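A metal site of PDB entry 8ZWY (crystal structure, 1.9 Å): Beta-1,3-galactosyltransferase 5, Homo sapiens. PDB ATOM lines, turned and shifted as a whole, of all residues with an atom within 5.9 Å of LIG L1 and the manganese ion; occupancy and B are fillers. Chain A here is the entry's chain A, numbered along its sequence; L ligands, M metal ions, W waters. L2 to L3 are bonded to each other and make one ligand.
An oxygen (O3) of LIG L1 lies within hydrogen-bond range of the side-chain amide oxygen (OE1) of Gln 39 (2.5 Å). An oxygen (O1) of LIG L1 is in hydrogen-bond range of the side-chain amino group (NZ) of Lys 104 (2.7 Å). The side-chain amino group (NZ) of Lys 167 lies within salt-bridge range of an oxygen (O12) of LIG L1, 2.9 Å away. The backbone NH (N) of Ser 127 is in hydrogen-bond range of an oxygen (O5) of LIG L1 (2.9 Å). OG of Ser 127 sits at hydrogen-bond distance from O3 of LIG L1. The side-chain hydroxyl of Tyr 98 lies within hydrogen-bond range of an oxygen (O11) of LIG L1 (2.9 Å). An oxygen (O5) of LIG L1 sits at hydrogen-bond distance from the backbone carbonyl oxygen (O) of Thr 34. The side-chain hydroxyl of Thr 34 lies within hydrogen-bond range of an oxygen (O5) of LIG L1. A nitrogen (N2) of LIG L1 sits at hydrogen-bond distance from the side-chain carboxylate (OD1) of Asp 96. N of Ser 35 lies close to O1 of LIG L1, at 3.3 Å.
The manganese ion is bound by an oxygen (O10) of LIG L1 (1.8 Å), an oxygen (O8) of LIG L1 (2.2 Å), the side-chain carboxylate (OD2) of Asp 126 (2.4 Å), a ring nitrogen (NE2) of His 255 (2.4 Å), the side-chain carboxylate (OD2) of Asp 128 (2.5 Å) and the side-chain carboxylate (OD1) of Asp 128 (2.6 Å). The manganese ion has six donor atoms within binding distance.
Ser 36 touches LIG L1 (N to O1, 3.6 Å). Val 97 touches LIG L1. Leu 101 touches LIG L1. Trp 168 touches LIG L1. Hydrophobic or aromatic side chains that line LIG L1: Tyr 98, Leu 101, Trp 168 and His 255. Along chain A the residues within 4 Å of LIG L1 span positions 34 to 255. The nearest printed residue that does not touch LIG L1 is Thr 125 (4.8 Å).
The nearest printed residue that does not touch the manganese ion is Thr 187 (5.0 Å).
The backbone NH of Asp 126 sits at hydrogen-bond distance from the backbone carbonyl oxygen of Thr 187, 3.0 Å away. O of Asp 128 is in hydrogen-bond range of N of Phe 256, at 3.2 Å. The side-chain amide oxygen (OE1) of Gln 39 is in hydrogen-bond range of the backbone NH (N) of Ser 36, 3.0 Å away. The side-chain carboxylate (OD2) of Asp 96 is in salt-bridge range of the side-chain amino group (NZ) of Lys 104, at 2.8 Å. The side-chain amino group (NZ) of Lys 104 lies within hydrogen-bond range of the backbone carbonyl oxygen (O) of Leu 66 (3.0 Å). The backbone carbonyl oxygen (O) of Thr 34 lies close to the backbone NH (N) of Ser 127. NE1 of Trp 168 sits at hydrogen-bond distance from OH of Tyr 98 (3.0 Å). O of Thr 125 sits at hydrogen-bond distance from N of Thr 34 (3.0 Å).
Water W6 bridges O7 of LIG L1 (2.7 Å) and NE2 of Gln 39 (3.5 Å). Water W3 lies within hydrogen-bond range of the backbone carbonyl oxygen of Asp 96 (2.9 Å) and an oxygen (O2) of LIG L1 (2.9 Å). Water W5 bridges the side-chain carboxylate of Asp 126 and an oxygen (O11) of LIG L1.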
ATOM      1  N   VAL A  33     -20.049  21.256  16.802  1.00  0.00           N
ATOM      2  CA  VAL A  33     -18.808  20.558  16.401  1.00  0.00           C
ATOM      3  C   VAL A  33     -17.681  20.782  17.433  1.00  0.00           C
ATOM      4  O   VAL A  33     -17.286  21.918  17.671  1.00  0.00           O
ATOM      5  CB  VAL A  33     -18.324  20.933  14.981  1.00  0.00           C
ATOM      6  CG1 VAL A  33     -17.139  20.093  14.548  1.00  0.00           C
ATOM      7  CG2 VAL A  33     -19.445  20.905  13.958  1.00  0.00           C
ATOM      8  N   THR A  34     -17.135  19.680  17.929  1.00  0.00           N
ATOM      9  CA  THR A  34     -16.015  19.747  18.864  1.00  0.00           C
ATOM     10  C   THR A  34     -14.722  19.801  18.071  1.00  0.00           C
ATOM     11  O   THR A  34     -14.572  19.081  17.084  1.00  0.00           O
ATOM     12  CB  THR A  34     -16.067  18.564  19.843  1.00  0.00           C
ATOM     13  OG1 THR A  34     -16.042  17.408  19.035  1.00  0.00           O
ATOM     14  CG2 THR A  34     -17.310  18.569  20.708  1.00  0.00           C
ATOM     15  N   SER A  35     -13.838  20.674  18.492  1.00  0.00           N
ATOM     16  CA  SER A  35     -12.496  20.762  17.873  1.00  0.00           C
ATOM     17  C   SER A  35     -11.572  21.450  18.891  1.00  0.00           C
ATOM     18  O   SER A  35     -12.081  22.272  19.651  1.00  0.00           O
ATOM     19  CB  SER A  35     -12.571  21.529  16.574  1.00  0.00           C
ATOM     20  OG  SER A  35     -12.572  22.937  16.738  1.00  0.00           O
ATOM     21  N   SER A  36     -10.280  21.151  18.852  1.00  0.00           N
ATOM     22  CA  SER A  36      -9.370  21.890  19.721  1.00  0.00           C
ATOM     23  C   SER A  36      -8.833  23.137  19.021  1.00  0.00           C
ATOM     24  O   SER A  36      -8.898  23.279  17.799  1.00  0.00           O
ATOM     25  CB  SER A  36      -8.237  20.996  20.214  1.00  0.00           C
ATOM     26  OG  SER A  36      -7.400  20.492  19.195  1.00  0.00           O
ATOM     27  N   GLN A  39      -6.912  23.035  15.652  1.00  0.00           N
ATOM     28  CA  GLN A  39      -7.528  22.365  14.527  1.00  0.00           C
ATOM     29  C   GLN A  39      -8.265  23.350  13.636  1.00  0.00           C
ATOM     30  O   GLN A  39      -9.432  23.137  13.288  1.00  0.00           O
ATOM     31  CB  GLN A  39      -8.457  21.259  15.033  1.00  0.00           C
ATOM     32  CG  GLN A  39      -7.721  20.034  15.619  1.00  0.00           C
ATOM     33  CD  GLN A  39      -8.631  18.882  16.067  1.00  0.00           C
ATOM     34  OE1 GLN A  39      -9.437  19.033  16.964  1.00  0.00           O
ATOM     35  NE2 GLN A  39      -8.457  17.717  15.461  1.00  0.00           N
ATOM     36  N   LEU A  66     -17.588  24.242  19.254  1.00  0.00           N
ATOM     37  CA  LEU A  66     -17.423  24.282  20.721  1.00  0.00           C
ATOM     38  C   LEU A  66     -15.928  24.345  21.044  1.00  0.00           C
ATOM     39  O   LEU A  66     -15.179  23.463  20.643  1.00  0.00           O
ATOM     40  CB  LEU A  66     -18.057  23.064  21.378  1.00  0.00           C
ATOM     41  CG  LEU A  66     -19.478  22.705  20.914  1.00  0.00           C
ATOM     42  CD1 LEU A  66     -19.966  21.483  21.659  1.00  0.00           C
ATOM     43  CD2 LEU A  66     -20.411  23.876  21.110  1.00  0.00           C
ATOM     44  N   ASP A  96      -9.264  23.322  27.498  1.00  0.00           N
ATOM     45  CA  ASP A  96      -9.685  22.475  26.358  1.00  0.00           C
ATOM     46  C   ASP A  96      -8.733  21.277  26.198  1.00  0.00           C
ATOM     47  O   ASP A  96      -7.758  21.413  25.472  1.00  0.00           O
ATOM     48  CB  ASP A  96      -9.856  23.357  25.137  1.00  0.00           C
ATOM     49  CG  ASP A  96     -10.743  22.769  24.054  1.00  0.00           C
ATOM     50  OD1 ASP A  96     -11.036  21.579  24.175  1.00  0.00           O
ATOM     51  OD2 ASP A  96     -11.148  23.503  23.141  1.00  0.00           O
ATOM     52  N   VAL A  97      -9.039  20.164  26.855  1.00  0.00           N
ATOM     53  CA  VAL A  97      -8.233  18.916  26.783  1.00  0.00           C
ATOM     54  C   VAL A  97      -9.178  17.705  26.639  1.00  0.00           C
ATOM     55  O   VAL A  97     -10.342  17.846  26.963  1.00  0.00           O
ATOM     56  CB  VAL A  97      -7.339  18.755  28.039  1.00  0.00           C
ATOM     57  CG1 VAL A  97      -6.223  19.781  28.062  1.00  0.00           C
ATOM     58  CG2 VAL A  97      -8.165  18.788  29.318  1.00  0.00           C
ATOM     59  N   TYR A  98      -8.665  16.582  26.151  1.00  0.00           N
ATOM     60  CA  TYR A  98      -9.506  15.373  25.915  1.00  0.00           C
ATOM     61  C   TYR A  98     -10.336  15.033  27.173  1.00  0.00           C
ATOM     62  O   TYR A  98     -11.534  14.848  27.015  1.00  0.00           O
ATOM     63  CB  TYR A  98      -8.712  14.167  25.411  1.00  0.00           C
ATOM     64  CG  TYR A  98      -9.616  13.101  24.788  1.00  0.00           C
ATOM     65  CD1 TYR A  98      -9.951  13.136  23.446  1.00  0.00           C
ATOM     66  CD2 TYR A  98     -10.142  12.085  25.568  1.00  0.00           C
ATOM     67  CE1 TYR A  98     -10.776  12.172  22.894  1.00  0.00           C
ATOM     68  CE2 TYR A  98     -10.974  11.114  25.026  1.00  0.00           C
ATOM     69  CZ  TYR A  98     -11.301  11.167  23.682  1.00  0.00           C
ATOM     70  OH  TYR A  98     -12.115  10.212  23.165  1.00  0.00           O
ATOM     71  N   LEU A 101     -13.676  16.951  27.722  1.00  0.00           N
ATOM     72  CA  LEU A 101     -14.741  16.863  26.680  1.00  0.00           C
ATOM     73  C   LEU A 101     -16.160  16.854  27.306  1.00  0.00           C
ATOM     74  O   LEU A 101     -17.080  17.323  26.667  1.00  0.00           O
ATOM     75  CB  LEU A 101     -14.442  15.646  25.816  1.00  0.00           C
ATOM     76  CG  LEU A 101     -13.393  15.855  24.727  1.00  0.00           C
ATOM     77  CD1 LEU A 101     -13.105  14.593  23.946  1.00  0.00           C
ATOM     78  CD2 LEU A 101     -13.792  16.992  23.807  1.00  0.00           C
ATOM     79  N   LYS A 104     -17.085  20.359  27.610  1.00  0.00           N
ATOM     80  CA  LYS A 104     -17.356  20.915  26.265  1.00  0.00           C
ATOM     81  C   LYS A 104     -18.789  20.532  25.857  1.00  0.00           C
ATOM     82  O   LYS A 104     -19.528  21.408  25.441  1.00  0.00           O
ATOM     83  CB  LYS A 104     -16.366  20.406  25.218  1.00  0.00           C
ATOM     84  CG  LYS A 104     -16.536  21.035  23.850  1.00  0.00           C
ATOM     85  CD  LYS A 104     -15.333  20.815  22.957  1.00  0.00           C
ATOM     86  CE  LYS A 104     -14.136  21.571  23.415  1.00  0.00           C
ATOM     87  NZ  LYS A 104     -13.240  21.825  22.291  1.00  0.00           N
ATOM     88  N   THR A 125     -21.167  16.522  17.192  1.00  0.00           N
ATOM     89  CA  THR A 125     -20.258  15.724  16.359  1.00  0.00           C
ATOM     90  C   THR A 125     -18.780  16.059  16.533  1.00  0.00           C
ATOM     91  O   THR A 125     -18.458  17.136  17.020  1.00  0.00           O
ATOM     92  CB  THR A 125     -20.636  15.801  14.870  1.00  0.00           C
ATOM     93  OG1 THR A 125     -19.864  14.852  14.142  1.00  0.00           O
ATOM     94  CG2 THR A 125     -20.430  17.184  14.285  1.00  0.00           C
ATOM     95  N   ASP A 126     -17.940  15.114  16.137  1.00  0.00           N
ATOM     96  CA  ASP A 126     -16.472  15.286  16.116  1.00  0.00           C
ATOM     97  C   ASP A 126     -16.084  16.091  14.874  1.00  0.00           C
ATOM     98  O   ASP A 126     -16.925  16.231  13.983  1.00  0.00           O
ATOM     99  CB  ASP A 126     -15.808  13.941  15.936  1.00  0.00           C
ATOM    100  CG  ASP A 126     -15.406  13.143  17.170  1.00  0.00           C
ATOM    101  OD1 ASP A 126     -16.121  13.140  18.161  1.00  0.00           O
ATOM    102  OD2 ASP A 126     -14.396  12.441  17.098  1.00  0.00           O
ATOM    103  N   SER A 127     -14.837  16.547  14.821  1.00  0.00           N
ATOM    104  CA  SER A 127     -14.308  17.316  13.673  1.00  0.00           C
ATOM    105  C   SER A 127     -13.807  16.364  12.569  1.00  0.00           C
ATOM    106  O   SER A 127     -13.746  16.817  11.430  1.00  0.00           O
ATOM    107  CB  SER A 127     -13.174  18.213  14.162  1.00  0.00           C
ATOM    108  OG  SER A 127     -12.267  17.511  14.995  1.00  0.00           O
ATOM    109  N   ASP A 128     -13.452  15.129  12.904  1.00  0.00           N
ATOM    110  CA  ASP A 128     -12.858  14.175  11.902  1.00  0.00           C
ATOM    111  C   ASP A 128     -14.002  13.332  11.330  1.00  0.00           C
ATOM    112  O   ASP A 128     -13.929  12.103  11.370  1.00  0.00           O
ATOM    113  CB  ASP A 128     -11.726  13.366  12.494  1.00  0.00           C
ATOM    114  CG  ASP A 128     -12.097  12.576  13.739  1.00  0.00           C
ATOM    115  OD1 ASP A 128     -13.085  12.936  14.406  1.00  0.00           O
ATOM    116  OD2 ASP A 128     -11.392  11.607  14.022  1.00  0.00           O
ATOM    117  N   MET A 129     -15.003  14.032  10.814  1.00  0.00           N
ATOM    118  CA  MET A 129     -16.224  13.313  10.414  1.00  0.00           C
ATOM    119  C   MET A 129     -16.786  13.813   9.081  1.00  0.00           C
ATOM    120  O   MET A 129     -16.471  14.929   8.679  1.00  0.00           O
ATOM    121  CB  MET A 129     -17.324  13.573  11.446  1.00  0.00           C
ATOM    122  CG  MET A 129     -17.044  13.073  12.847  1.00  0.00           C
ATOM    123  SD  MET A 129     -17.337  11.300  12.955  1.00  0.00           S
ATOM    124  CE  MET A 129     -19.105  11.280  12.595  1.00  0.00           C
ATOM    125  N   LYS A 167      -6.879   5.029  26.023  1.00  0.00           N
ATOM    126  CA  LYS A 167      -7.457   6.395  25.945  1.00  0.00           C
ATOM    127  C   LYS A 167      -8.760   6.479  26.756  1.00  0.00           C
ATOM    128  O   LYS A 167      -9.003   7.500  27.383  1.00  0.00           O
ATOM    129  CB  LYS A 167      -7.804   6.635  24.483  1.00  0.00           C
ATOM    130  CG  LYS A 167      -8.138   8.054  24.068  1.00  0.00           C
ATOM    131  CD  LYS A 167      -8.632   8.109  22.628  1.00  0.00           C
ATOM    132  CE  LYS A 167      -8.844   9.502  22.156  1.00  0.00           C
ATOM    133  NZ  LYS A 167      -8.299   9.711  20.810  1.00  0.00           N
ATOM    134  N   TRP A 168      -9.571   5.435  26.723  1.00  0.00           N
ATOM    135  CA  TRP A 168     -10.896   5.475  27.394  1.00  0.00           C
ATOM    136  C   TRP A 168     -10.849   4.780  28.764  1.00  0.00           C
ATOM    137  O   TRP A 168     -11.893   4.455  29.323  1.00  0.00           O
ATOM    138  CB  TRP A 168     -11.932   4.865  26.456  1.00  0.00           C
ATOM    139  CG  TRP A 168     -12.041   5.591  25.143  1.00  0.00           C
ATOM    140  CD1 TRP A 168     -12.206   6.927  24.944  1.00  0.00           C
ATOM    141  CD2 TRP A 168     -11.990   4.992  23.826  1.00  0.00           C
ATOM    142  NE1 TRP A 168     -12.242   7.200  23.603  1.00  0.00           N
ATOM    143  CE2 TRP A 168     -12.128   6.033  22.897  1.00  0.00           C
ATOM    144  CE3 TRP A 168     -11.844   3.674  23.366  1.00  0.00           C
ATOM    145  CZ2 TRP A 168     -12.119   5.812  21.528  1.00  0.00           C
ATOM    146  CZ3 TRP A 168     -11.842   3.457  22.016  1.00  0.00           C
ATOM    147  CH2 TRP A 168     -11.984   4.512  21.104  1.00  0.00           C
ATOM    148  N   THR A 187     -18.834  10.183  18.600  1.00  0.00           N
ATOM    149  CA  THR A 187     -18.435  10.634  17.250  1.00  0.00           C
ATOM    150  C   THR A 187     -19.516  11.495  16.620  1.00  0.00           C
ATOM    151  O   THR A 187     -19.189  12.416  15.875  1.00  0.00           O
ATOM    152  CB  THR A 187     -18.117   9.418  16.371  1.00  0.00           C
ATOM    153  OG1 THR A 187     -19.197   8.506  16.323  1.00  0.00           O
ATOM    154  CG2 THR A 187     -16.853   8.706  16.848  1.00  0.00           C
ATOM    155  N   HIS A 255     -16.813   8.351  10.489  1.00  0.00           N
ATOM    156  CA  HIS A 255     -15.676   8.840  11.286  1.00  0.00           C
ATOM    157  C   HIS A 255     -14.357   8.589  10.543  1.00  0.00           C
ATOM    158  O   HIS A 255     -14.398   8.078   9.422  1.00  0.00           O
ATOM    159  CB  HIS A 255     -15.749   8.110  12.629  1.00  0.00           C
ATOM    160  CG  HIS A 255     -14.785   8.463  13.667  1.00  0.00           C
ATOM    161  ND1 HIS A 255     -14.170   7.466  14.383  1.00  0.00           N
ATOM    162  CD2 HIS A 255     -14.330   9.609  14.134  1.00  0.00           C
ATOM    163  CE1 HIS A 255     -13.359   8.009  15.262  1.00  0.00           C
ATOM    164  NE2 HIS A 255     -13.455   9.295  15.123  1.00  0.00           N
ATOM    165  N   PHE A 256     -13.229   8.981  11.151  1.00  0.00           N
ATOM    166  CA  PHE A 256     -11.887   8.730  10.559  1.00  0.00           C
ATOM    167  C   PHE A 256     -11.723   9.475   9.235  1.00  0.00           C
ATOM    168  O   PHE A 256     -11.142   8.917   8.307  1.00  0.00           O
ATOM    169  CB  PHE A 256     -11.649   7.219  10.455  1.00  0.00           C
ATOM    170  CG  PHE A 256     -11.562   6.517  11.809  1.00  0.00           C
ATOM    171  CD1 PHE A 256     -10.831   7.073  12.841  1.00  0.00           C
ATOM    172  CD2 PHE A 256     -12.225   5.325  12.031  1.00  0.00           C
ATOM    173  CE1 PHE A 256     -10.748   6.440  14.067  1.00  0.00           C
ATOM    174  CE2 PHE A 256     -12.142   4.693  13.257  1.00  0.00           C
ATOM    175  CZ  PHE A 256     -11.408   5.257  14.266  1.00  0.00           C
HETATM  176  N1  LIG L   1     -11.236  17.460  20.893  1.00  0.00           N
HETATM  177  C1  LIG L   1     -11.455  18.721  21.481  1.00  0.00           C
HETATM  178  N2  LIG L   1     -10.481  19.135  22.355  1.00  0.00           N
HETATM  179  C2  LIG L   1      -9.340  18.448  22.713  1.00  0.00           C
HETATM  180  C3  LIG L   1      -9.193  17.151  22.095  1.00  0.00           C
HETATM  181  C4  LIG L   1     -10.114  16.723  21.201  1.00  0.00           C
HETATM  182  O1  LIG L   1     -12.410  19.440  21.208  1.00  0.00           O
HETATM  183  O2  LIG L   1      -8.566  18.948  23.534  1.00  0.00           O
HETATM  184  C5  LIG L   1     -12.213  16.974  19.915  1.00  0.00           C
HETATM  185  C6  LIG L   1     -11.612  16.480  18.607  1.00  0.00           C
HETATM  186  O3  LIG L   1     -11.355  17.543  17.713  1.00  0.00           O
HETATM  187  C7  LIG L   1     -12.735  15.578  18.113  1.00  0.00           C
HETATM  188  C8  LIG L   1     -13.190  14.919  19.426  1.00  0.00           C
HETATM  189  O4  LIG L   1     -12.820  15.847  20.472  1.00  0.00           O
HETATM  190  O5  LIG L   1     -13.753  16.357  17.505  1.00  0.00           O
HETATM  191  C9  LIG L   1     -12.588  13.570  19.740  1.00  0.00           C
HETATM  192  O6  LIG L   1     -11.162  13.681  19.509  1.00  0.00           O
HETATM  193  P1  LIG L   1     -10.402  12.627  18.616  1.00  0.00           P
HETATM  194  O7  LIG L   1      -8.991  13.032  18.572  1.00  0.00           O
HETATM  195  O8  LIG L   1     -11.063  12.489  17.257  1.00  0.00           O
HETATM  196  O9  LIG L   1     -10.574  11.260  19.341  1.00  0.00           O
HETATM  197  P2  LIG L   1     -11.565  10.032  19.129  1.00  0.00           P
HETATM  198  O10 LIG L   1     -12.201   9.954  17.525  1.00  0.00           O
HETATM  199  O11 LIG L   1     -12.543  10.206  20.328  1.00  0.00           O
HETATM  200  O12 LIG L   1     -10.718   8.844  19.541  1.00  0.00           O
HETATM  201  C1  LG2 L   2     -14.121  -0.241  20.935  1.00  0.00           C
HETATM  202  C2  LG2 L   2     -14.930   1.052  20.853  1.00  0.00           C
HETATM  203  C3  LG2 L   2     -15.181   1.626  22.242  1.00  0.00           C
HETATM  204  C4  LG2 L   2     -15.743   0.570  23.161  1.00  0.00           C
HETATM  205  C5  LG2 L   2     -14.790  -0.605  23.193  1.00  0.00           C
HETATM  206  C6  LG2 L   2     -15.255  -1.728  24.098  1.00  0.00           C
HETATM  207  C7  LG2 L   2     -13.206  -1.894  19.544  1.00  0.00           C
HETATM  208  O1  LG2 L   2     -14.092  -0.794  19.654  1.00  0.00           O
HETATM  209  O2  LG2 L   2     -14.262   2.014  20.052  1.00  0.00           O
HETATM  210  O3  LG2 L   2     -16.064   2.732  22.155  1.00  0.00           O
HETATM  211  O4  LG2 L   2     -16.997   0.156  22.674  1.00  0.00           O
HETATM  212  O5  LG2 L   2     -14.682  -1.143  21.861  1.00  0.00           O
HETATM  213  O6  LG2 L   2     -14.348  -2.806  24.111  1.00  0.00           O
HETATM  214  C1  LG3 L   3     -15.707   3.784  22.990  1.00  0.00           C
HETATM  215  C2  LG3 L   3     -16.214   5.092  22.394  1.00  0.00           C
HETATM  216  C3  LG3 L   3     -15.910   6.242  23.350  1.00  0.00           C
HETATM  217  C4  LG3 L   3     -16.504   5.935  24.713  1.00  0.00           C
HETATM  218  C5  LG3 L   3     -15.865   4.636  25.192  1.00  0.00           C
HETATM  219  C6  LG3 L   3     -16.303   4.205  26.567  1.00  0.00           C
HETATM  220  C7  LG3 L   3     -16.304   5.302  19.951  1.00  0.00           C
HETATM  221  C8  LG3 L   3     -15.497   5.224  18.698  1.00  0.00           C
HETATM  222  N1  LG3 L   3     -15.621   5.327  21.093  1.00  0.00           N
HETATM  223  O1  LG3 L   3     -16.392   7.467  22.827  1.00  0.00           O
HETATM  224  O2  LG3 L   3     -16.208   6.997  25.610  1.00  0.00           O
HETATM  225  O3  LG3 L   3     -16.247   3.591  24.290  1.00  0.00           O
HETATM  226  O4  LG3 L   3     -15.648   3.000  26.920  1.00  0.00           O
HETATM  227  O5  LG3 L   3     -17.524   5.334  19.929  1.00  0.00           O
HETATM  228 MN    MN M   1     -12.514  11.213  16.235  1.00  0.00          MN
HETATM  229  O   HOH W   1     -10.140   9.414  15.554  1.00  0.00           O
HETATM  230  O   HOH W   2      -9.725  13.793  15.630  1.00  0.00           O
HETATM  231  O   HOH W   3      -5.942  20.179  23.631  1.00  0.00           O
HETATM  232  O   HOH W   4     -13.513   7.646  18.965  1.00  0.00           O
HETATM  233  O   HOH W   5     -15.592  11.243  20.542  1.00  0.00           O
HETATM  234  O   HOH W   6      -8.097  15.570  18.200  1.00  0.00           O
